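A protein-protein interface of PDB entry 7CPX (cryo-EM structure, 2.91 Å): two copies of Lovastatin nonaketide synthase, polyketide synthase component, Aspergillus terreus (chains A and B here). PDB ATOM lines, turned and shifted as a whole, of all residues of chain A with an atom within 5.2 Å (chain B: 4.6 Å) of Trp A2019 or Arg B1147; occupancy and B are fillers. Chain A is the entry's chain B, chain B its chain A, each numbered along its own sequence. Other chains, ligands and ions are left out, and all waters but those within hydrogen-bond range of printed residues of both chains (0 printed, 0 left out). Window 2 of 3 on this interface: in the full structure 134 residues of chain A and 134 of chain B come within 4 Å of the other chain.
Hydrophobic or aromatic side chains of chain B that line the printed part of chain A: Ile B1227. Hydrophobic or aromatic side chains of chain A that line the printed part of chain B: Trp A2019 and His A2020. Among the printed residues, Asp or Glu carboxylates within 4 Å of a Lys or Arg side-chain nitrogen of the other chain: Arg A2023 with Glu B1106 (3.1 Å).
No position is printed for both chains.
The side-chain carboxylate (OE2) of Glu B1106 sits at hydrogen-bond distance from a ring nitrogen (ND1) of His A2020, at 2.7 Å. NH2 of Arg A2023 is in salt-bridge range of OE1 of Glu B1106 (3.1 Å).
Printed residues of chain B within 4 Å of Trp A2019: Glu B1106 (3.97 Å), Arg B1147 (3.3 Å), Ile B1227 (3.6 Å), Thr B1229 (3.99 Å) and Asp B1239 (3.7 Å). Printed residues of chain B within 4 Å of His A2020: Glu B1106. Printed residues of chain B within 4 Å of Arg A2023: Glu B1106. Of the printed residues of chain A, Glu B1106 touches Trp A2019 (3.97 Å), His A2020 (2.7 Å) and Arg A2023 (3.1 Å). Of chain A, only Trp A2019 comes within 4 Å of Arg B1147. Thr B1226 touches none of the printed residues of chain A. Of the printed residues of chain A, Asp B1239 touches Thr A2017, Asp A2018 and Trp A2019. The nearest printed residue of chain B that does not touch Trp A2019 is His B2200 (5.7 Å).
Asp B1239 touches Thr A2017 (OD2 to CB, 3.5 Å). Asp A2018 touches Asp B1239. Glu B1106 touches Trp A2019 (OE2 to CZ3, 3.97 Å). CZ2 of Trp A2019 touches NH1 of Arg B1147 (3.3 Å). Trp A2019 touches Ile B1227. Thr B1229 touches Trp A2019. OD2 of Asp B1239 touches CB of Trp A2019, 3.7 Å away.
ND1 of His B1109 sits close to NH1 of Arg B1147. O of Asp B1239 is in hydrogen-bond range of N of Ile B1227, 2.9 Å away. OG1 of Thr A2017 lies within hydrogen-bond range of N of His A2020 (3.1 Å). OD2 of Asp A2018 is in salt-bridge range of NH1 of Arg A2022, at 2.9 Å. NH2 of Arg A2023 sits close to ND1 of His A2020 (3.4 Å).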
ATOM      1  N   THR A2017     -16.594   9.531  -8.198  1.00  0.00           N
ATOM      2  CA  THR A2017     -15.791  10.651  -7.734  1.00  0.00           C
ATOM      3  C   THR A2017     -14.308  10.387  -7.967  1.00  0.00           C
ATOM      4  O   THR A2017     -13.854   9.240  -8.000  1.00  0.00           O
ATOM      5  CB  THR A2017     -16.035  10.910  -6.248  1.00  0.00           C
ATOM      6  OG1 THR A2017     -15.501   9.826  -5.478  1.00  0.00           O
ATOM      7  CG2 THR A2017     -17.521  11.039  -5.968  1.00  0.00           C
ATOM      8  N   ASP A2018     -13.548  11.473  -8.121  1.00  0.00           N
ATOM      9  CA  ASP A2018     -12.110  11.341  -8.317  1.00  0.00           C
ATOM     10  C   ASP A2018     -11.441  10.695  -7.113  1.00  0.00           C
ATOM     11  O   ASP A2018     -10.473   9.942  -7.270  1.00  0.00           O
ATOM     12  CB  ASP A2018     -11.490  12.710  -8.595  1.00  0.00           C
ATOM     13  CG  ASP A2018     -11.694  13.683  -7.454  1.00  0.00           C
ATOM     14  OD1 ASP A2018     -12.716  13.565  -6.746  1.00  0.00           O
ATOM     15  OD2 ASP A2018     -10.831  14.566  -7.265  1.00  0.00           O
ATOM     16  N   TRP A2019     -11.933  10.980  -5.906  1.00  0.00           N
ATOM     17  CA  TRP A2019     -11.370  10.359  -4.712  1.00  0.00           C
ATOM     18  C   TRP A2019     -11.557   8.847  -4.742  1.00  0.00           C
ATOM     19  O   TRP A2019     -10.641   8.090  -4.401  1.00  0.00           O
ATOM     20  CB  TRP A2019     -12.015  10.956  -3.464  1.00  0.00           C
ATOM     21  CG  TRP A2019     -11.614  10.279  -2.199  1.00  0.00           C
ATOM     22  CD1 TRP A2019     -10.583  10.621  -1.377  1.00  0.00           C
ATOM     23  CD2 TRP A2019     -12.239   9.137  -1.605  1.00  0.00           C
ATOM     24  NE1 TRP A2019     -10.525   9.763  -0.308  1.00  0.00           N
ATOM     25  CE2 TRP A2019     -11.531   8.840  -0.424  1.00  0.00           C
ATOM     26  CE3 TRP A2019     -13.327   8.335  -1.957  1.00  0.00           C
ATOM     27  CZ2 TRP A2019     -11.878   7.779   0.406  1.00  0.00           C
ATOM     28  CZ3 TRP A2019     -13.670   7.280  -1.132  1.00  0.00           C
ATOM     29  CH2 TRP A2019     -12.947   7.012   0.036  1.00  0.00           C
ATOM     30  N   HIS A2020     -12.741   8.387  -5.150  1.00  0.00           N
ATOM     31  CA  HIS A2020     -12.976   6.952  -5.258  1.00  0.00           C
ATOM     32  C   HIS A2020     -12.046   6.324  -6.287  1.00  0.00           C
ATOM     33  O   HIS A2020     -11.519   5.225  -6.073  1.00  0.00           O
ATOM     34  CB  HIS A2020     -14.436   6.688  -5.623  1.00  0.00           C
ATOM     35  CG  HIS A2020     -14.733   5.254  -5.925  1.00  0.00           C
ATOM     36  ND1 HIS A2020     -14.845   4.292  -4.944  1.00  0.00           N
ATOM     37  CD2 HIS A2020     -14.941   4.615  -7.101  1.00  0.00           C
ATOM     38  CE1 HIS A2020     -15.110   3.124  -5.502  1.00  0.00           C
ATOM     39  NE2 HIS A2020     -15.172   3.293  -6.811  1.00  0.00           N
ATOM     40  N   LEU A2021     -11.840   7.006  -7.415  1.00  0.00           N
ATOM     41  CA  LEU A2021     -10.924   6.495  -8.429  1.00  0.00           C
ATOM     42  C   LEU A2021      -9.506   6.398  -7.883  1.00  0.00           C
ATOM     43  O   LEU A2021      -8.812   5.400  -8.110  1.00  0.00           O
ATOM     44  CB  LEU A2021     -10.967   7.390  -9.665  1.00  0.00           C
ATOM     45  CG  LEU A2021     -12.336   7.485 -10.342  1.00  0.00           C
ATOM     46  CD1 LEU A2021     -12.326   8.554 -11.416  1.00  0.00           C
ATOM     47  CD2 LEU A2021     -12.748   6.143 -10.925  1.00  0.00           C
ATOM     48  N   ARG A2022      -9.058   7.421  -7.154  1.00  0.00           N
ATOM     49  CA  ARG A2022      -7.756   7.342  -6.503  1.00  0.00           C
ATOM     50  C   ARG A2022      -7.693   6.143  -5.570  1.00  0.00           C
ATOM     51  O   ARG A2022      -6.678   5.438  -5.515  1.00  0.00           O
ATOM     52  CB  ARG A2022      -7.473   8.628  -5.726  1.00  0.00           C
ATOM     53  CG  ARG A2022      -7.113   9.820  -6.592  1.00  0.00           C
ATOM     54  CD  ARG A2022      -6.777  11.040  -5.752  1.00  0.00           C
ATOM     55  NE  ARG A2022      -6.284  12.147  -6.564  1.00  0.00           N
ATOM     56  CZ  ARG A2022      -7.055  13.057  -7.147  1.00  0.00           C
ATOM     57  NH1 ARG A2022      -8.372  13.026  -7.032  1.00  0.00           N
ATOM     58  NH2 ARG A2022      -6.487  14.024  -7.863  1.00  0.00           N
ATOM     59  N   ARG A2023      -8.773   5.895  -4.831  1.00  0.00           N
ATOM     60  CA  ARG A2023      -8.788   4.778  -3.894  1.00  0.00           C
ATOM     61  C   ARG A2023      -8.670   3.442  -4.617  1.00  0.00           C
ATOM     62  O   ARG A2023      -7.939   2.552  -4.168  1.00  0.00           O
ATOM     63  CB  ARG A2023     -10.064   4.817  -3.055  1.00  0.00           C
ATOM     64  CG  ARG A2023     -10.106   3.770  -1.956  1.00  0.00           C
ATOM     65  CD  ARG A2023     -11.397   3.839  -1.163  1.00  0.00           C
ATOM     66  NE  ARG A2023     -12.542   3.364  -1.931  1.00  0.00           N
ATOM     67  CZ  ARG A2023     -12.837   2.085  -2.122  1.00  0.00           C
ATOM     68  NH1 ARG A2023     -12.074   1.120  -1.638  1.00  0.00           N
ATOM     69  NH2 ARG A2023     -13.924   1.768  -2.819  1.00  0.00           N
ATOM     70  N   VAL A2024      -9.375   3.279  -5.733  1.00  0.00           N
ATOM     71  CA  VAL A2024      -9.499   1.983  -6.388  1.00  0.00           C
ATOM     72  C   VAL A2024      -8.523   1.834  -7.550  1.00  0.00           C
ATOM     73  O   VAL A2024      -7.917   0.774  -7.714  1.00  0.00           O
ATOM     74  CB  VAL A2024     -10.953   1.754  -6.856  1.00  0.00           C
ATOM     75  CG1 VAL A2024     -11.913   1.900  -5.690  1.00  0.00           C
ATOM     76  CG2 VAL A2024     -11.318   2.710  -7.979  1.00  0.00           C
ATOM     77  N   GLU B1106     -19.952   3.958  -0.325  1.00  0.00           N
ATOM     78  CA  GLU B1106     -18.888   3.206   0.313  1.00  0.00           C
ATOM     79  C   GLU B1106     -19.446   2.430   1.504  1.00  0.00           C
ATOM     80  O   GLU B1106     -20.589   2.617   1.930  1.00  0.00           O
ATOM     81  CB  GLU B1106     -17.760   4.138   0.750  1.00  0.00           C
ATOM     82  CG  GLU B1106     -17.089   4.878  -0.398  1.00  0.00           C
ATOM     83  CD  GLU B1106     -16.413   3.946  -1.385  1.00  0.00           C
ATOM     84  OE1 GLU B1106     -16.241   2.752  -1.057  1.00  0.00           O
ATOM     85  OE2 GLU B1106     -16.053   4.405  -2.489  1.00  0.00           O
ATOM     86  N   HIS B1109     -18.344   3.787   6.454  1.00  0.00           N
ATOM     87  CA  HIS B1109     -16.985   3.874   6.980  1.00  0.00           C
ATOM     88  C   HIS B1109     -16.920   3.353   8.413  1.00  0.00           C
ATOM     89  O   HIS B1109     -17.731   3.743   9.262  1.00  0.00           O
ATOM     90  CB  HIS B1109     -16.499   5.324   6.913  1.00  0.00           C
ATOM     91  CG  HIS B1109     -15.010   5.463   6.920  1.00  0.00           C
ATOM     92  ND1 HIS B1109     -14.211   4.963   5.915  1.00  0.00           N
ATOM     93  CD2 HIS B1109     -14.173   6.033   7.818  1.00  0.00           C
ATOM     94  CE1 HIS B1109     -12.946   5.225   6.189  1.00  0.00           C
ATOM     95  NE2 HIS B1109     -12.895   5.873   7.339  1.00  0.00           N
ATOM     96  N   MET B1112     -16.407   5.515  13.487  1.00  0.00           N
ATOM     97  CA  MET B1112     -16.593   6.957  13.441  1.00  0.00           C
ATOM     98  C   MET B1112     -17.173   7.370  14.784  1.00  0.00           C
ATOM     99  O   MET B1112     -18.266   6.930  15.150  1.00  0.00           O
ATOM    100  CB  MET B1112     -17.507   7.356  12.288  1.00  0.00           C
ATOM    101  CG  MET B1112     -17.316   6.529  11.029  1.00  0.00           C
ATOM    102  SD  MET B1112     -18.167   7.226   9.604  1.00  0.00           S
ATOM    103  CE  MET B1112     -16.927   8.373   9.013  1.00  0.00           C
ATOM    104  N   GLN B1142     -21.547  10.562  12.514  1.00  0.00           N
ATOM    105  CA  GLN B1142     -20.372  10.006  13.165  1.00  0.00           C
ATOM    106  C   GLN B1142     -19.190  10.170  12.225  1.00  0.00           C
ATOM    107  O   GLN B1142     -19.303   9.878  11.031  1.00  0.00           O
ATOM    108  CB  GLN B1142     -20.590   8.536  13.532  1.00  0.00           C
ATOM    109  CG  GLN B1142     -21.048   7.655  12.380  1.00  0.00           C
ATOM    110  CD  GLN B1142     -22.551   7.484  12.340  1.00  0.00           C
ATOM    111  OE1 GLN B1142     -23.300   8.460  12.309  1.00  0.00           O
ATOM    112  NE2 GLN B1142     -23.003   6.236  12.349  1.00  0.00           N
ATOM    113  N   ARG B1143     -18.063  10.630  12.765  1.00  0.00           N
ATOM    114  CA  ARG B1143     -16.930  11.048  11.949  1.00  0.00           C
ATOM    115  C   ARG B1143     -15.645  10.367  12.395  1.00  0.00           C
ATOM    116  O   ARG B1143     -15.458  10.071  13.576  1.00  0.00           O
ATOM    117  CB  ARG B1143     -16.725  12.564  12.014  1.00  0.00           C
ATOM    118  CG  ARG B1143     -16.206  13.062  13.359  1.00  0.00           C
ATOM    119  CD  ARG B1143     -15.804  14.516  13.299  1.00  0.00           C
ATOM    120  NE  ARG B1143     -14.791  14.758  12.279  1.00  0.00           N
ATOM    121  CZ  ARG B1143     -13.508  14.453  12.416  1.00  0.00           C
ATOM    122  NH1 ARG B1143     -13.048  13.883  13.517  1.00  0.00           N
ATOM    123  NH2 ARG B1143     -12.667  14.721  11.423  1.00  0.00           N
ATOM    124  N   ALA B1144     -14.751  10.147  11.434  1.00  0.00           N
ATOM    125  CA  ALA B1144     -13.403   9.670  11.714  1.00  0.00           C
ATOM    126  C   ALA B1144     -12.634   9.583  10.405  1.00  0.00           C
ATOM    127  O   ALA B1144     -13.222   9.544   9.320  1.00  0.00           O
ATOM    128  CB  ALA B1144     -13.409   8.310  12.407  1.00  0.00           C
ATOM    129  N   ASP B1145     -11.306   9.547  10.524  1.00  0.00           N
ATOM    130  CA  ASP B1145     -10.421   9.353   9.379  1.00  0.00           C
ATOM    131  C   ASP B1145     -10.731  10.352   8.269  1.00  0.00           C
ATOM    132  O   ASP B1145     -10.789  10.005   7.088  1.00  0.00           O
ATOM    133  CB  ASP B1145     -10.515   7.921   8.857  1.00  0.00           C
ATOM    134  CG  ASP B1145     -10.156   6.891   9.909  1.00  0.00           C
ATOM    135  OD1 ASP B1145      -9.793   7.292  11.035  1.00  0.00           O
ATOM    136  OD2 ASP B1145     -10.240   5.682   9.612  1.00  0.00           O
ATOM    137  N   LEU B1146     -10.934  11.610   8.654  1.00  0.00           N
ATOM    138  CA  LEU B1146     -11.270  12.664   7.700  1.00  0.00           C
ATOM    139  C   LEU B1146     -12.517  12.288   6.905  1.00  0.00           C
ATOM    140  O   LEU B1146     -12.603  12.516   5.697  1.00  0.00           O
ATOM    141  CB  LEU B1146     -10.093  12.949   6.766  1.00  0.00           C
ATOM    142  CG  LEU B1146     -10.184  14.220   5.921  1.00  0.00           C
ATOM    143  CD1 LEU B1146     -10.388  15.434   6.804  1.00  0.00           C
ATOM    144  CD2 LEU B1146      -8.938  14.383   5.068  1.00  0.00           C
ATOM    145  N   ARG B1147     -13.490  11.699   7.593  1.00  0.00           N
ATOM    146  CA  ARG B1147     -14.693  11.202   6.947  1.00  0.00           C
ATOM    147  C   ARG B1147     -15.852  11.301   7.925  1.00  0.00           C
ATOM    148  O   ARG B1147     -15.658  11.377   9.141  1.00  0.00           O
ATOM    149  CB  ARG B1147     -14.514   9.756   6.478  1.00  0.00           C
ATOM    150  CG  ARG B1147     -14.714   9.557   4.994  1.00  0.00           C
ATOM    151  CD  ARG B1147     -14.149   8.226   4.535  1.00  0.00           C
ATOM    152  NE  ARG B1147     -12.711   8.295   4.303  1.00  0.00           N
ATOM    153  CZ  ARG B1147     -12.007   7.361   3.678  1.00  0.00           C
ATOM    154  NH1 ARG B1147     -12.577   6.265   3.204  1.00  0.00           N
ATOM    155  NH2 ARG B1147     -10.699   7.534   3.519  1.00  0.00           N
ATOM    156  N   ALA B1148     -17.065  11.298   7.379  1.00  0.00           N
ATOM    157  CA  ALA B1148     -18.259  11.300   8.206  1.00  0.00           C
ATOM    158  C   ALA B1148     -19.330  10.467   7.525  1.00  0.00           C
ATOM    159  O   ALA B1148     -19.262  10.187   6.327  1.00  0.00           O
ATOM    160  CB  ALA B1148     -18.770  12.721   8.473  1.00  0.00           C
ATOM    161  N   ALA B1183     -17.210  15.825   8.910  1.00  0.00           N
ATOM    162  CA  ALA B1183     -16.022  15.033   8.612  1.00  0.00           C
ATOM    163  C   ALA B1183     -14.760  15.856   8.816  1.00  0.00           C
ATOM    164  O   ALA B1183     -13.724  15.333   9.240  1.00  0.00           O
ATOM    165  CB  ALA B1183     -16.084  14.503   7.180  1.00  0.00           C
ATOM    166  N   THR B1226     -19.632  10.753   3.540  1.00  0.00           N
ATOM    167  CA  THR B1226     -18.980  11.952   3.035  1.00  0.00           C
ATOM    168  C   THR B1226     -17.496  11.897   3.352  1.00  0.00           C
ATOM    169  O   THR B1226     -17.102  11.520   4.462  1.00  0.00           O
ATOM    170  CB  THR B1226     -19.607  13.214   3.637  1.00  0.00           C
ATOM    171  OG1 THR B1226     -18.767  14.344   3.372  1.00  0.00           O
ATOM    172  CG2 THR B1226     -19.785  13.054   5.130  1.00  0.00           C
ATOM    173  N   ILE B1227     -16.688  12.282   2.371  1.00  0.00           N
ATOM    174  CA  ILE B1227     -15.242  12.376   2.500  1.00  0.00           C
ATOM    175  C   ILE B1227     -14.877  13.849   2.506  1.00  0.00           C
ATOM    176  O   ILE B1227     -15.286  14.597   1.610  1.00  0.00           O
ATOM    177  CB  ILE B1227     -14.516  11.657   1.349  1.00  0.00           C
ATOM    178  CG1 ILE B1227     -15.379  10.545   0.741  1.00  0.00           C
ATOM    179  CG2 ILE B1227     -13.180  11.113   1.826  1.00  0.00           C
ATOM    180  CD1 ILE B1227     -15.711   9.417   1.681  1.00  0.00           C
ATOM    181  N   THR B1229     -12.377  15.498   1.397  1.00  0.00           N
ATOM    182  CA  THR B1229     -11.248  15.203   0.520  1.00  0.00           C
ATOM    183  C   THR B1229     -10.088  16.157   0.761  1.00  0.00           C
ATOM    184  O   THR B1229      -8.930  15.732   0.841  1.00  0.00           O
ATOM    185  CB  THR B1229     -11.691  15.266  -0.943  1.00  0.00           C
ATOM    186  OG1 THR B1229     -12.263  16.550  -1.218  1.00  0.00           O
ATOM    187  CG2 THR B1229     -12.716  14.186  -1.231  1.00  0.00           C
ATOM    188  N   ASP B1239     -16.666  15.213  -0.847  1.00  0.00           N
ATOM    189  CA  ASP B1239     -17.501  14.405  -1.722  1.00  0.00           C
ATOM    190  C   ASP B1239     -18.572  13.729  -0.882  1.00  0.00           C
ATOM    191  O   ASP B1239     -18.254  13.030   0.083  1.00  0.00           O
ATOM    192  CB  ASP B1239     -16.671  13.358  -2.467  1.00  0.00           C
ATOM    193  CG  ASP B1239     -15.548  13.971  -3.277  1.00  0.00           C
ATOM    194  OD1 ASP B1239     -15.371  15.205  -3.212  1.00  0.00           O
ATOM    195  OD2 ASP B1239     -14.839  13.219  -3.978  1.00  0.00           O
ATOM    196  N   ARG B2174      -3.014   6.117   9.982  1.00  0.00           N
ATOM    197  CA  ARG B2174      -3.468   6.362   8.619  1.00  0.00           C
ATOM    198  C   ARG B2174      -2.804   7.610   8.051  1.00  0.00           C
ATOM    199  O   ARG B2174      -2.431   7.645   6.873  1.00  0.00           O
ATOM    200  CB  ARG B2174      -4.993   6.473   8.563  1.00  0.00           C
ATOM    201  CG  ARG B2174      -5.575   7.800   9.017  1.00  0.00           C
ATOM    202  CD  ARG B2174      -7.058   7.869   8.711  1.00  0.00           C
ATOM    203  NE  ARG B2174      -7.321   7.736   7.282  1.00  0.00           N
ATOM    204  CZ  ARG B2174      -7.264   8.733   6.410  1.00  0.00           C
ATOM    205  NH1 ARG B2174      -6.955   9.963   6.784  1.00  0.00           N
ATOM    206  NH2 ARG B2174      -7.519   8.490   5.128  1.00  0.00           N
ATOM    207  N   HIS B2200      -8.186  -0.920   4.697  1.00  0.00           N
ATOM    208  CA  HIS B2200      -8.354   0.459   4.246  1.00  0.00           C
ATOM    209  C   HIS B2200      -7.026   1.201   4.257  1.00  0.00           C
ATOM    210  O   HIS B2200      -6.674   1.884   3.288  1.00  0.00           O
ATOM    211  CB  HIS B2200      -9.373   1.179   5.130  1.00  0.00           C
ATOM    212  CG  HIS B2200      -9.207   2.667   5.146  1.00  0.00           C
ATOM    213  ND1 HIS B2200      -9.342   3.445   4.016  1.00  0.00           N
ATOM    214  CD2 HIS B2200      -8.913   3.520   6.155  1.00  0.00           C
ATOM    215  CE1 HIS B2200      -9.139   4.712   4.329  1.00  0.00           C
ATOM    216  NE2 HIS B2200      -8.878   4.785   5.621  1.00  0.00           N
